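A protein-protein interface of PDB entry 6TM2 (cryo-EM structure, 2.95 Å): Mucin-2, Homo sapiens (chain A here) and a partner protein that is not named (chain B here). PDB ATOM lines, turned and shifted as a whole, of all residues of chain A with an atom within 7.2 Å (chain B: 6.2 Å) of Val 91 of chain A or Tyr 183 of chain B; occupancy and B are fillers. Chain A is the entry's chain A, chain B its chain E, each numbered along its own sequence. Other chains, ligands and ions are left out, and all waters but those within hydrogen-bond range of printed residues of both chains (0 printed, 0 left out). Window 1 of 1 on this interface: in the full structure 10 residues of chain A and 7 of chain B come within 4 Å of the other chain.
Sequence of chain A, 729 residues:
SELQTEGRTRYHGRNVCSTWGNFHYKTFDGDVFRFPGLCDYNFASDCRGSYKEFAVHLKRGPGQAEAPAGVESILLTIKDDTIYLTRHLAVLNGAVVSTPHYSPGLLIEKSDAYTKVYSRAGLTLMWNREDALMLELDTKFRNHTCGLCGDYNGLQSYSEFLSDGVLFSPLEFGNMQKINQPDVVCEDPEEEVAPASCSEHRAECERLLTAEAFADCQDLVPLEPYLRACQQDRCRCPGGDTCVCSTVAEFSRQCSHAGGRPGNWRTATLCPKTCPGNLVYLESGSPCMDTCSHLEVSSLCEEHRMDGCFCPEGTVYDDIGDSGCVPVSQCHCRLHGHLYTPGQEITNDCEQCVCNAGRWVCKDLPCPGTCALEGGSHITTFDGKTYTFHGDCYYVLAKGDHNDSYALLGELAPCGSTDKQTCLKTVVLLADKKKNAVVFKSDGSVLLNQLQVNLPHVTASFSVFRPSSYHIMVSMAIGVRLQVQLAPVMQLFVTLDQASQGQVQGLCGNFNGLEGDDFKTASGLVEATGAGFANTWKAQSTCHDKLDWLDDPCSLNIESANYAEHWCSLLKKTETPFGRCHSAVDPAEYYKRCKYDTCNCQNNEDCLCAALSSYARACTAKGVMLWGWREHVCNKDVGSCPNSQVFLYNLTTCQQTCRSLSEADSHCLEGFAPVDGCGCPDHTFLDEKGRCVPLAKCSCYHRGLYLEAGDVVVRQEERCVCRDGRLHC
O of Thr 82 of chain A sits at hydrogen-bond distance from N of Asn 93 of chain A (3.1 Å).
SG of Cys 168 of chain B is disulfide-bonded to SG of Cys 182 of chain B.
N of Tyr 84 of chain A sits at hydrogen-bond distance from O of Val 91 of chain A (2.8 Å).
The side-chain hydroxyl (OG1) of Thr 86 of chain A lies within hydrogen-bond range of the backbone carbonyl oxygen (O) of Leu 89 of chain A (3.0 Å).
OE1 of Gln 156 of chain B is in hydrogen-bond range of N of Tyr 183 of chain B.
Among the printed residues, pairs that only touch across the chains: Leu 89 of chain A with His 154 of chain B (3.5 Å), Val 91 of chain A with Tyr 183 of chain B (3.5 Å), Gly 94 of chain A with Phe 179 of chain B (3.5 Å), Thr 82 of chain A with Phe 179 of chain B (3.6 Å), Val 96 of chain A with Tyr 183 of chain B (3.6 Å), Tyr 84 of chain A with Phe 179 of chain B (3.7 Å), Leu 89 of chain A with Tyr 183 of chain B (3.8 Å), Val 91 of chain A with Phe 179 of chain B (3.8 Å) and Asn 93 of chain A with Phe 179 of chain B (3.8 Å).
Of the printed residues of chain B, Tyr 84 of chain A touches Phe 179.
Printed residues of chain B within 4 Å of Leu 89 of chain A: His 154 and Tyr 183.
Val 91 of chain A touches two residues of chain B.
Cys 168 of chain B touches none of the printed residues of chain A.
Of chain A, only Leu 89 (3.8 Å), Val 91 (3.5 Å) and Val 96 (3.6 Å) come within 4 Å of Tyr 183 of chain B.
The nearest printed residue of chain B that does not touch Val 91 of chain A is His 154 of chain B (7.3 Å).
The nearest printed residue of chain A that does not touch His 154 of chain B is Val 96 of chain A (4.9 Å).
Printed residues of chain A that touch a printed residue of chain B: Thr 82, Tyr 84, Leu 89, Val 91, Asn 93, Gly 94 and Val 96.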
ATOM      1  N   LEU A  75     -15.490  -5.739  21.146  1.00  0.00           N
ATOM      2  CA  LEU A  75     -15.616  -5.180  19.812  1.00  0.00           C
ATOM      3  C   LEU A  75     -14.890  -6.093  18.840  1.00  0.00           C
ATOM      4  O   LEU A  75     -13.748  -6.485  19.085  1.00  0.00           O
ATOM      5  CB  LEU A  75     -15.048  -3.770  19.755  1.00  0.00           C
ATOM      6  CG  LEU A  75     -15.293  -3.034  18.453  1.00  0.00           C
ATOM      7  CD1 LEU A  75     -16.776  -2.832  18.300  1.00  0.00           C
ATOM      8  CD2 LEU A  75     -14.579  -1.718  18.489  1.00  0.00           C
ATOM      9  N   LEU A  76     -15.554  -6.424  17.739  1.00  0.00           N
ATOM     10  CA  LEU A  76     -15.090  -7.449  16.814  1.00  0.00           C
ATOM     11  C   LEU A  76     -15.418  -7.018  15.398  1.00  0.00           C
ATOM     12  O   LEU A  76     -16.577  -6.734  15.090  1.00  0.00           O
ATOM     13  CB  LEU A  76     -15.735  -8.792  17.163  1.00  0.00           C
ATOM     14  CG  LEU A  76     -15.456 -10.066  16.385  1.00  0.00           C
ATOM     15  CD1 LEU A  76     -15.471 -11.210  17.311  1.00  0.00           C
ATOM     16  CD2 LEU A  76     -16.603 -10.269  15.463  1.00  0.00           C
ATOM     17  N   THR A  82     -18.900  -4.979  11.708  1.00  0.00           N
ATOM     18  CA  THR A  82     -18.477  -4.783  13.082  1.00  0.00           C
ATOM     19  C   THR A  82     -19.536  -5.348  14.010  1.00  0.00           C
ATOM     20  O   THR A  82     -20.712  -4.992  13.902  1.00  0.00           O
ATOM     21  CB  THR A  82     -18.265  -3.297  13.363  1.00  0.00           C
ATOM     22  OG1 THR A  82     -17.344  -2.760  12.411  1.00  0.00           O
ATOM     23  CG2 THR A  82     -17.687  -3.105  14.730  1.00  0.00           C
ATOM     24  N   ILE A  83     -19.125  -6.218  14.923  1.00  0.00           N
ATOM     25  CA  ILE A  83     -20.021  -6.808  15.905  1.00  0.00           C
ATOM     26  C   ILE A  83     -19.659  -6.248  17.271  1.00  0.00           C
ATOM     27  O   ILE A  83     -18.491  -6.271  17.668  1.00  0.00           O
ATOM     28  CB  ILE A  83     -19.948  -8.343  15.889  1.00  0.00           C
ATOM     29  CG1 ILE A  83     -20.372  -8.849  14.523  1.00  0.00           C
ATOM     30  CG2 ILE A  83     -20.870  -8.937  16.916  1.00  0.00           C
ATOM     31  CD1 ILE A  83     -20.120 -10.282  14.318  1.00  0.00           C
ATOM     32  N   TYR A  84     -20.658  -5.732  17.972  1.00  0.00           N
ATOM     33  CA  TYR A  84     -20.508  -5.117  19.284  1.00  0.00           C
ATOM     34  C   TYR A  84     -21.332  -5.893  20.297  1.00  0.00           C
ATOM     35  O   TYR A  84     -22.563  -5.869  20.253  1.00  0.00           O
ATOM     36  CB  TYR A  84     -20.923  -3.651  19.217  1.00  0.00           C
ATOM     37  CG  TYR A  84     -20.981  -2.943  20.536  1.00  0.00           C
ATOM     38  CD1 TYR A  84     -19.833  -2.680  21.264  1.00  0.00           C
ATOM     39  CD2 TYR A  84     -22.184  -2.462  21.013  1.00  0.00           C
ATOM     40  CE1 TYR A  84     -19.894  -2.015  22.461  1.00  0.00           C
ATOM     41  CE2 TYR A  84     -22.256  -1.791  22.198  1.00  0.00           C
ATOM     42  CZ  TYR A  84     -21.110  -1.567  22.919  1.00  0.00           C
ATOM     43  OH  TYR A  84     -21.194  -0.896  24.112  1.00  0.00           O
ATOM     44  N   LEU A  85     -20.653  -6.571  21.211  1.00  0.00           N
ATOM     45  CA  LEU A  85     -21.283  -7.435  22.195  1.00  0.00           C
ATOM     46  C   LEU A  85     -21.252  -6.754  23.549  1.00  0.00           C
ATOM     47  O   LEU A  85     -20.192  -6.328  24.003  1.00  0.00           O
ATOM     48  CB  LEU A  85     -20.553  -8.774  22.296  1.00  0.00           C
ATOM     49  CG  LEU A  85     -20.485  -9.687  21.083  1.00  0.00           C
ATOM     50  CD1 LEU A  85     -19.606 -10.876  21.398  1.00  0.00           C
ATOM     51  CD2 LEU A  85     -21.862 -10.128  20.683  1.00  0.00           C
ATOM     52  N   THR A  86     -22.401  -6.654  24.190  1.00  0.00           N
ATOM     53  CA  THR A  86     -22.475  -6.267  25.587  1.00  0.00           C
ATOM     54  C   THR A  86     -23.102  -7.403  26.379  1.00  0.00           C
ATOM     55  O   THR A  86     -23.298  -8.509  25.874  1.00  0.00           O
ATOM     56  CB  THR A  86     -23.264  -4.978  25.780  1.00  0.00           C
ATOM     57  OG1 THR A  86     -24.585  -5.143  25.261  1.00  0.00           O
ATOM     58  CG2 THR A  86     -22.605  -3.849  25.089  1.00  0.00           C
ATOM     59  N   LEU A  89     -27.142  -7.254  24.960  1.00  0.00           N
ATOM     60  CA  LEU A  89     -27.522  -7.210  23.558  1.00  0.00           C
ATOM     61  C   LEU A  89     -26.309  -7.310  22.652  1.00  0.00           C
ATOM     62  O   LEU A  89     -25.184  -7.009  23.043  1.00  0.00           O
ATOM     63  CB  LEU A  89     -28.359  -5.957  23.255  1.00  0.00           C
ATOM     64  CG  LEU A  89     -27.958  -4.536  23.657  1.00  0.00           C
ATOM     65  CD1 LEU A  89     -26.987  -3.855  22.756  1.00  0.00           C
ATOM     66  CD2 LEU A  89     -29.218  -3.750  23.674  1.00  0.00           C
ATOM     67  N   ALA A  90     -26.567  -7.761  21.431  1.00  0.00           N
ATOM     68  CA  ALA A  90     -25.565  -7.939  20.394  1.00  0.00           C
ATOM     69  C   ALA A  90     -25.953  -7.077  19.208  1.00  0.00           C
ATOM     70  O   ALA A  90     -27.093  -7.135  18.748  1.00  0.00           O
ATOM     71  CB  ALA A  90     -25.459  -9.403  19.974  1.00  0.00           C
ATOM     72  N   VAL A  91     -25.011  -6.281  18.719  1.00  0.00           N
ATOM     73  CA  VAL A  91     -25.266  -5.270  17.700  1.00  0.00           C
ATOM     74  C   VAL A  91     -24.372  -5.551  16.507  1.00  0.00           C
ATOM     75  O   VAL A  91     -23.148  -5.615  16.644  1.00  0.00           O
ATOM     76  CB  VAL A  91     -25.032  -3.854  18.245  1.00  0.00           C
ATOM     77  CG1 VAL A  91     -25.108  -2.848  17.152  1.00  0.00           C
ATOM     78  CG2 VAL A  91     -26.063  -3.537  19.256  1.00  0.00           C
ATOM     79  N   LEU A  92     -24.981  -5.722  15.345  1.00  0.00           N
ATOM     80  CA  LEU A  92     -24.282  -5.906  14.080  1.00  0.00           C
ATOM     81  C   LEU A  92     -24.542  -4.692  13.208  1.00  0.00           C
ATOM     82  O   LEU A  92     -25.678  -4.480  12.774  1.00  0.00           O
ATOM     83  CB  LEU A  92     -24.744  -7.177  13.379  1.00  0.00           C
ATOM     84  CG  LEU A  92     -24.218  -7.485  11.976  1.00  0.00           C
ATOM     85  CD1 LEU A  92     -22.734  -7.673  11.934  1.00  0.00           C
ATOM     86  CD2 LEU A  92     -24.902  -8.710  11.450  1.00  0.00           C
ATOM     87  N   ASN A  93     -23.483  -3.916  12.953  1.00  0.00           N
ATOM     88  CA  ASN A  93     -23.496  -2.743  12.072  1.00  0.00           C
ATOM     89  C   ASN A  93     -24.516  -1.701  12.523  1.00  0.00           C
ATOM     90  O   ASN A  93     -25.228  -1.117  11.709  1.00  0.00           O
ATOM     91  CB  ASN A  93     -23.743  -3.131  10.613  1.00  0.00           C
ATOM     92  CG  ASN A  93     -22.601  -3.910  10.012  1.00  0.00           C
ATOM     93  OD1 ASN A  93     -21.436  -3.594  10.229  1.00  0.00           O
ATOM     94  ND2 ASN A  93     -22.931  -4.941   9.250  1.00  0.00           N
ATOM     95  N   GLY A  94     -24.598  -1.471  13.826  1.00  0.00           N
ATOM     96  CA  GLY A  94     -25.449  -0.434  14.359  1.00  0.00           C
ATOM     97  C   GLY A  94     -26.877  -0.841  14.620  1.00  0.00           C
ATOM     98  O   GLY A  94     -27.629  -0.052  15.198  1.00  0.00           O
ATOM     99  N   ALA A  95     -27.273  -2.042  14.219  1.00  0.00           N
ATOM    100  CA  ALA A  95     -28.617  -2.552  14.417  1.00  0.00           C
ATOM    101  C   ALA A  95     -28.595  -3.724  15.385  1.00  0.00           C
ATOM    102  O   ALA A  95     -27.697  -4.566  15.330  1.00  0.00           O
ATOM    103  CB  ALA A  95     -29.231  -2.994  13.093  1.00  0.00           C
ATOM    104  N   VAL A  96     -29.586  -3.771  16.272  1.00  0.00           N
ATOM    105  CA  VAL A  96     -29.724  -4.878  17.210  1.00  0.00           C
ATOM    106  C   VAL A  96     -30.159  -6.124  16.454  1.00  0.00           C
ATOM    107  O   VAL A  96     -31.041  -6.066  15.595  1.00  0.00           O
ATOM    108  CB  VAL A  96     -30.732  -4.497  18.309  1.00  0.00           C
ATOM    109  CG1 VAL A  96     -30.980  -5.634  19.255  1.00  0.00           C
ATOM    110  CG2 VAL A  96     -30.231  -3.326  19.079  1.00  0.00           C
ATOM    111  N   VAL A  97     -29.526  -7.260  16.739  1.00  0.00           N
ATOM    112  CA  VAL A  97     -29.885  -8.520  16.101  1.00  0.00           C
ATOM    113  C   VAL A  97     -30.656  -9.388  17.083  1.00  0.00           C
ATOM    114  O   VAL A  97     -30.397  -9.376  18.292  1.00  0.00           O
ATOM    115  CB  VAL A  97     -28.663  -9.273  15.534  1.00  0.00           C
ATOM    116  CG1 VAL A  97     -28.027  -8.471  14.441  1.00  0.00           C
ATOM    117  CG2 VAL A  97     -27.652  -9.583  16.589  1.00  0.00           C
ATOM    118  N   ILE A 108     -24.344 -15.888  14.663  1.00  0.00           N
ATOM    119  CA  ILE A 108     -24.330 -15.234  15.965  1.00  0.00           C
ATOM    120  C   ILE A 108     -25.478 -15.824  16.767  1.00  0.00           C
ATOM    121  O   ILE A 108     -26.643 -15.526  16.491  1.00  0.00           O
ATOM    122  CB  ILE A 108     -24.491 -13.711  15.847  1.00  0.00           C
ATOM    123  CG1 ILE A 108     -23.381 -13.096  15.008  1.00  0.00           C
ATOM    124  CG2 ILE A 108     -24.483 -13.066  17.219  1.00  0.00           C
ATOM    125  CD1 ILE A 108     -23.653 -11.675  14.659  1.00  0.00           C
ATOM    126  N   HIS B 116     -38.059   5.449  11.862  1.00  0.00           N
ATOM    127  CA  HIS B 116     -36.867   4.623  11.772  1.00  0.00           C
ATOM    128  C   HIS B 116     -35.637   5.479  12.027  1.00  0.00           C
ATOM    129  O   HIS B 116     -35.671   6.698  11.830  1.00  0.00           O
ATOM    130  CB  HIS B 116     -36.764   3.945  10.399  1.00  0.00           C
ATOM    131  CG  HIS B 116     -37.856   2.959  10.140  1.00  0.00           C
ATOM    132  ND1 HIS B 116     -37.872   1.703  10.704  1.00  0.00           N
ATOM    133  CD2 HIS B 116     -38.992   3.058   9.411  1.00  0.00           C
ATOM    134  CE1 HIS B 116     -38.959   1.061  10.314  1.00  0.00           C
ATOM    135  NE2 HIS B 116     -39.656   1.862   9.531  1.00  0.00           N
ATOM    136  N   PRO B 117     -34.542   4.872  12.489  1.00  0.00           N
ATOM    137  CA  PRO B 117     -33.296   5.644  12.612  1.00  0.00           C
ATOM    138  C   PRO B 117     -32.627   5.925  11.278  1.00  0.00           C
ATOM    139  O   PRO B 117     -32.048   7.004  11.098  1.00  0.00           O
ATOM    140  CB  PRO B 117     -32.428   4.748  13.505  1.00  0.00           C
ATOM    141  CG  PRO B 117     -33.392   3.891  14.229  1.00  0.00           C
ATOM    142  CD  PRO B 117     -34.487   3.626  13.267  1.00  0.00           C
ATOM    143  N   ASP B 125     -35.520   8.785  16.572  1.00  0.00           N
ATOM    144  CA  ASP B 125     -36.698   7.930  16.489  1.00  0.00           C
ATOM    145  C   ASP B 125     -37.741   8.480  17.447  1.00  0.00           C
ATOM    146  O   ASP B 125     -37.487   8.577  18.651  1.00  0.00           O
ATOM    147  CB  ASP B 125     -36.349   6.482  16.831  1.00  0.00           C
ATOM    148  CG  ASP B 125     -37.436   5.508  16.444  1.00  0.00           C
ATOM    149  OD1 ASP B 125     -38.476   5.931  15.913  1.00  0.00           O
ATOM    150  OD2 ASP B 125     -37.250   4.302  16.667  1.00  0.00           O
ATOM    151  N   SER B 143     -38.400  -2.477  21.884  1.00  0.00           N
ATOM    152  CA  SER B 143     -37.613  -2.451  20.660  1.00  0.00           C
ATOM    153  C   SER B 143     -38.169  -3.441  19.650  1.00  0.00           C
ATOM    154  O   SER B 143     -38.871  -4.390  19.994  1.00  0.00           O
ATOM    155  CB  SER B 143     -36.145  -2.782  20.931  1.00  0.00           C
ATOM    156  OG  SER B 143     -35.395  -2.784  19.730  1.00  0.00           O
ATOM    157  N   HIS B 154     -31.026  -1.545  27.103  1.00  0.00           N
ATOM    158  CA  HIS B 154     -30.497  -1.022  25.853  1.00  0.00           C
ATOM    159  C   HIS B 154     -29.341  -0.063  26.048  1.00  0.00           C
ATOM    160  O   HIS B 154     -28.479   0.034  25.171  1.00  0.00           O
ATOM    161  CB  HIS B 154     -31.585  -0.320  25.050  1.00  0.00           C
ATOM    162  CG  HIS B 154     -32.568  -1.249  24.425  1.00  0.00           C
ATOM    163  ND1 HIS B 154     -32.253  -2.017  23.327  1.00  0.00           N
ATOM    164  CD2 HIS B 154     -33.865  -1.507  24.705  1.00  0.00           C
ATOM    165  CE1 HIS B 154     -33.306  -2.726  22.972  1.00  0.00           C
ATOM    166  NE2 HIS B 154     -34.300  -2.433  23.790  1.00  0.00           N
ATOM    167  N   GLY B 155     -29.306   0.665  27.158  1.00  0.00           N
ATOM    168  CA  GLY B 155     -28.239   1.594  27.431  1.00  0.00           C
ATOM    169  C   GLY B 155     -28.379   2.947  26.770  1.00  0.00           C
ATOM    170  O   GLY B 155     -27.703   3.892  27.184  1.00  0.00           O
ATOM    171  N   GLN B 156     -29.215   3.066  25.747  1.00  0.00           N
ATOM    172  CA  GLN B 156     -29.478   4.367  25.165  1.00  0.00           C
ATOM    173  C   GLN B 156     -30.346   5.188  26.103  1.00  0.00           C
ATOM    174  O   GLN B 156     -31.099   4.647  26.915  1.00  0.00           O
ATOM    175  CB  GLN B 156     -30.141   4.221  23.797  1.00  0.00           C
ATOM    176  CG  GLN B 156     -29.198   3.714  22.725  1.00  0.00           C
ATOM    177  CD  GLN B 156     -29.849   3.613  21.370  1.00  0.00           C
ATOM    178  OE1 GLN B 156     -31.057   3.744  21.240  1.00  0.00           O
ATOM    179  NE2 GLN B 156     -29.034   3.468  20.340  1.00  0.00           N
ATOM    180  N   PHE B 166     -42.602   9.120  22.625  1.00  0.00           N
ATOM    181  CA  PHE B 166     -41.251   8.578  22.673  1.00  0.00           C
ATOM    182  C   PHE B 166     -40.303   9.515  21.939  1.00  0.00           C
ATOM    183  O   PHE B 166     -40.642  10.033  20.874  1.00  0.00           O
ATOM    184  CB  PHE B 166     -41.205   7.178  22.048  1.00  0.00           C
ATOM    185  CG  PHE B 166     -39.848   6.552  22.074  1.00  0.00           C
ATOM    186  CD1 PHE B 166     -39.333   6.044  23.251  1.00  0.00           C
ATOM    187  CD2 PHE B 166     -39.087   6.467  20.922  1.00  0.00           C
ATOM    188  CE1 PHE B 166     -38.088   5.475  23.282  1.00  0.00           C
ATOM    189  CE2 PHE B 166     -37.840   5.900  20.950  1.00  0.00           C
ATOM    190  CZ  PHE B 166     -37.342   5.408  22.132  1.00  0.00           C
ATOM    191  N   CYS B 168     -36.091   9.709  20.906  1.00  0.00           N
ATOM    192  CA  CYS B 168     -34.685   9.330  20.867  1.00  0.00           C
ATOM    193  C   CYS B 168     -33.981  10.299  19.931  1.00  0.00           C
ATOM    194  O   CYS B 168     -34.471  10.568  18.830  1.00  0.00           O
ATOM    195  CB  CYS B 168     -34.493   7.877  20.393  1.00  0.00           C
ATOM    196  SG  CYS B 168     -32.795   7.217  20.467  1.00  0.00           S
ATOM    197  N   PHE B 179     -21.122   2.980  17.446  1.00  0.00           N
ATOM    198  CA  PHE B 179     -21.913   3.281  16.262  1.00  0.00           C
ATOM    199  C   PHE B 179     -22.642   4.611  16.357  1.00  0.00           C
ATOM    200  O   PHE B 179     -22.682   5.353  15.374  1.00  0.00           O
ATOM    201  CB  PHE B 179     -22.923   2.162  16.008  1.00  0.00           C
ATOM    202  CG  PHE B 179     -22.293   0.839  15.703  1.00  0.00           C
ATOM    203  CD1 PHE B 179     -21.746   0.590  14.463  1.00  0.00           C
ATOM    204  CD2 PHE B 179     -22.281  -0.166  16.646  1.00  0.00           C
ATOM    205  CE1 PHE B 179     -21.170  -0.626  14.184  1.00  0.00           C
ATOM    206  CE2 PHE B 179     -21.711  -1.382  16.370  1.00  0.00           C
ATOM    207  CZ  PHE B 179     -21.158  -1.611  15.140  1.00  0.00           C
ATOM    208  N   LEU B 181     -26.108   5.508  17.074  1.00  0.00           N
ATOM    209  CA  LEU B 181     -27.390   5.598  16.395  1.00  0.00           C
ATOM    210  C   LEU B 181     -28.473   5.111  17.341  1.00  0.00           C
ATOM    211  O   LEU B 181     -28.207   4.314  18.243  1.00  0.00           O
ATOM    212  CB  LEU B 181     -27.421   4.762  15.111  1.00  0.00           C
ATOM    213  CG  LEU B 181     -26.537   5.155  13.929  1.00  0.00           C
ATOM    214  CD1 LEU B 181     -26.611   4.115  12.840  1.00  0.00           C
ATOM    215  CD2 LEU B 181     -26.953   6.494  13.389  1.00  0.00           C
ATOM    216  N   CYS B 182     -29.693   5.600  17.143  1.00  0.00           N
ATOM    217  CA  CYS B 182     -30.810   5.049  17.896  1.00  0.00           C
ATOM    218  C   CYS B 182     -31.131   3.647  17.402  1.00  0.00           C
ATOM    219  O   CYS B 182     -30.855   3.285  16.258  1.00  0.00           O
ATOM    220  CB  CYS B 182     -32.055   5.936  17.789  1.00  0.00           C
ATOM    221  SG  CYS B 182     -31.981   7.528  18.627  1.00  0.00           S
ATOM    222  N   TYR B 183     -31.690   2.842  18.294  1.00  0.00           N
ATOM    223  CA  TYR B 183     -32.221   1.550  17.904  1.00  0.00           C
ATOM    224  C   TYR B 183     -33.632   1.769  17.364  1.00  0.00           C
ATOM    225  O   TYR B 183     -34.157   2.881  17.371  1.00  0.00           O
ATOM    226  CB  TYR B 183     -32.185   0.586  19.091  1.00  0.00           C
ATOM    227  CG  TYR B 183     -30.788   0.239  19.567  1.00  0.00           C
ATOM    228  CD1 TYR B 183     -29.689   0.352  18.728  1.00  0.00           C
ATOM    229  CD2 TYR B 183     -30.561  -0.105  20.890  1.00  0.00           C
ATOM    230  CE1 TYR B 183     -28.427   0.075  19.177  1.00  0.00           C
ATOM    231  CE2 TYR B 183     -29.297  -0.376  21.348  1.00  0.00           C
ATOM    232  CZ  TYR B 183     -28.235  -0.284  20.485  1.00  0.00           C
ATOM    233  OH  TYR B 183     -26.966  -0.548  20.927  1.00  0.00           O
ATOM    234  N   ASP B 184     -34.261   0.710  16.885  1.00  0.00           N
ATOM    235  CA  ASP B 184     -35.583   0.813  16.286  1.00  0.00           C
ATOM    236  C   ASP B 184     -36.604   0.433  17.347  1.00  0.00           C
ATOM    237  O   ASP B 184     -36.601  -0.699  17.836  1.00  0.00           O
ATOM    238  CB  ASP B 184     -35.681  -0.089  15.060  1.00  0.00           C
ATOM    239  CG  ASP B 184     -36.888   0.204  14.207  1.00  0.00           C
ATOM    240  OD1 ASP B 184     -37.682   1.101  14.550  1.00  0.00           O
ATOM    241  OD2 ASP B 184     -37.040  -0.471  13.172  1.00  0.00           O
ATOM    242  N   TYR B 185     -37.468   1.374  17.700  1.00  0.00           N
ATOM    243  CA  TYR B 185     -38.403   1.235  18.804  1.00  0.00           C
ATOM    244  C   TYR B 185     -39.840   1.193  18.299  1.00  0.00           C
ATOM    245  O   TYR B 185     -40.133   1.526  17.148  1.00  0.00           O
ATOM    246  CB  TYR B 185     -38.222   2.387  19.791  1.00  0.00           C
ATOM    247  CG  TYR B 185     -36.929   2.371  20.573  1.00  0.00           C
ATOM    248  CD1 TYR B 185     -36.821   1.655  21.755  1.00  0.00           C
ATOM    249  CD2 TYR B 185     -35.810   3.053  20.117  1.00  0.00           C
ATOM    250  CE1 TYR B 185     -35.651   1.648  22.473  1.00  0.00           C
ATOM    251  CE2 TYR B 185     -34.634   3.045  20.831  1.00  0.00           C
ATOM    252  CZ  TYR B 185     -34.565   2.344  22.007  1.00  0.00           C
ATOM    253  OH  TYR B 185     -33.394   2.333  22.721  1.00  0.00           O
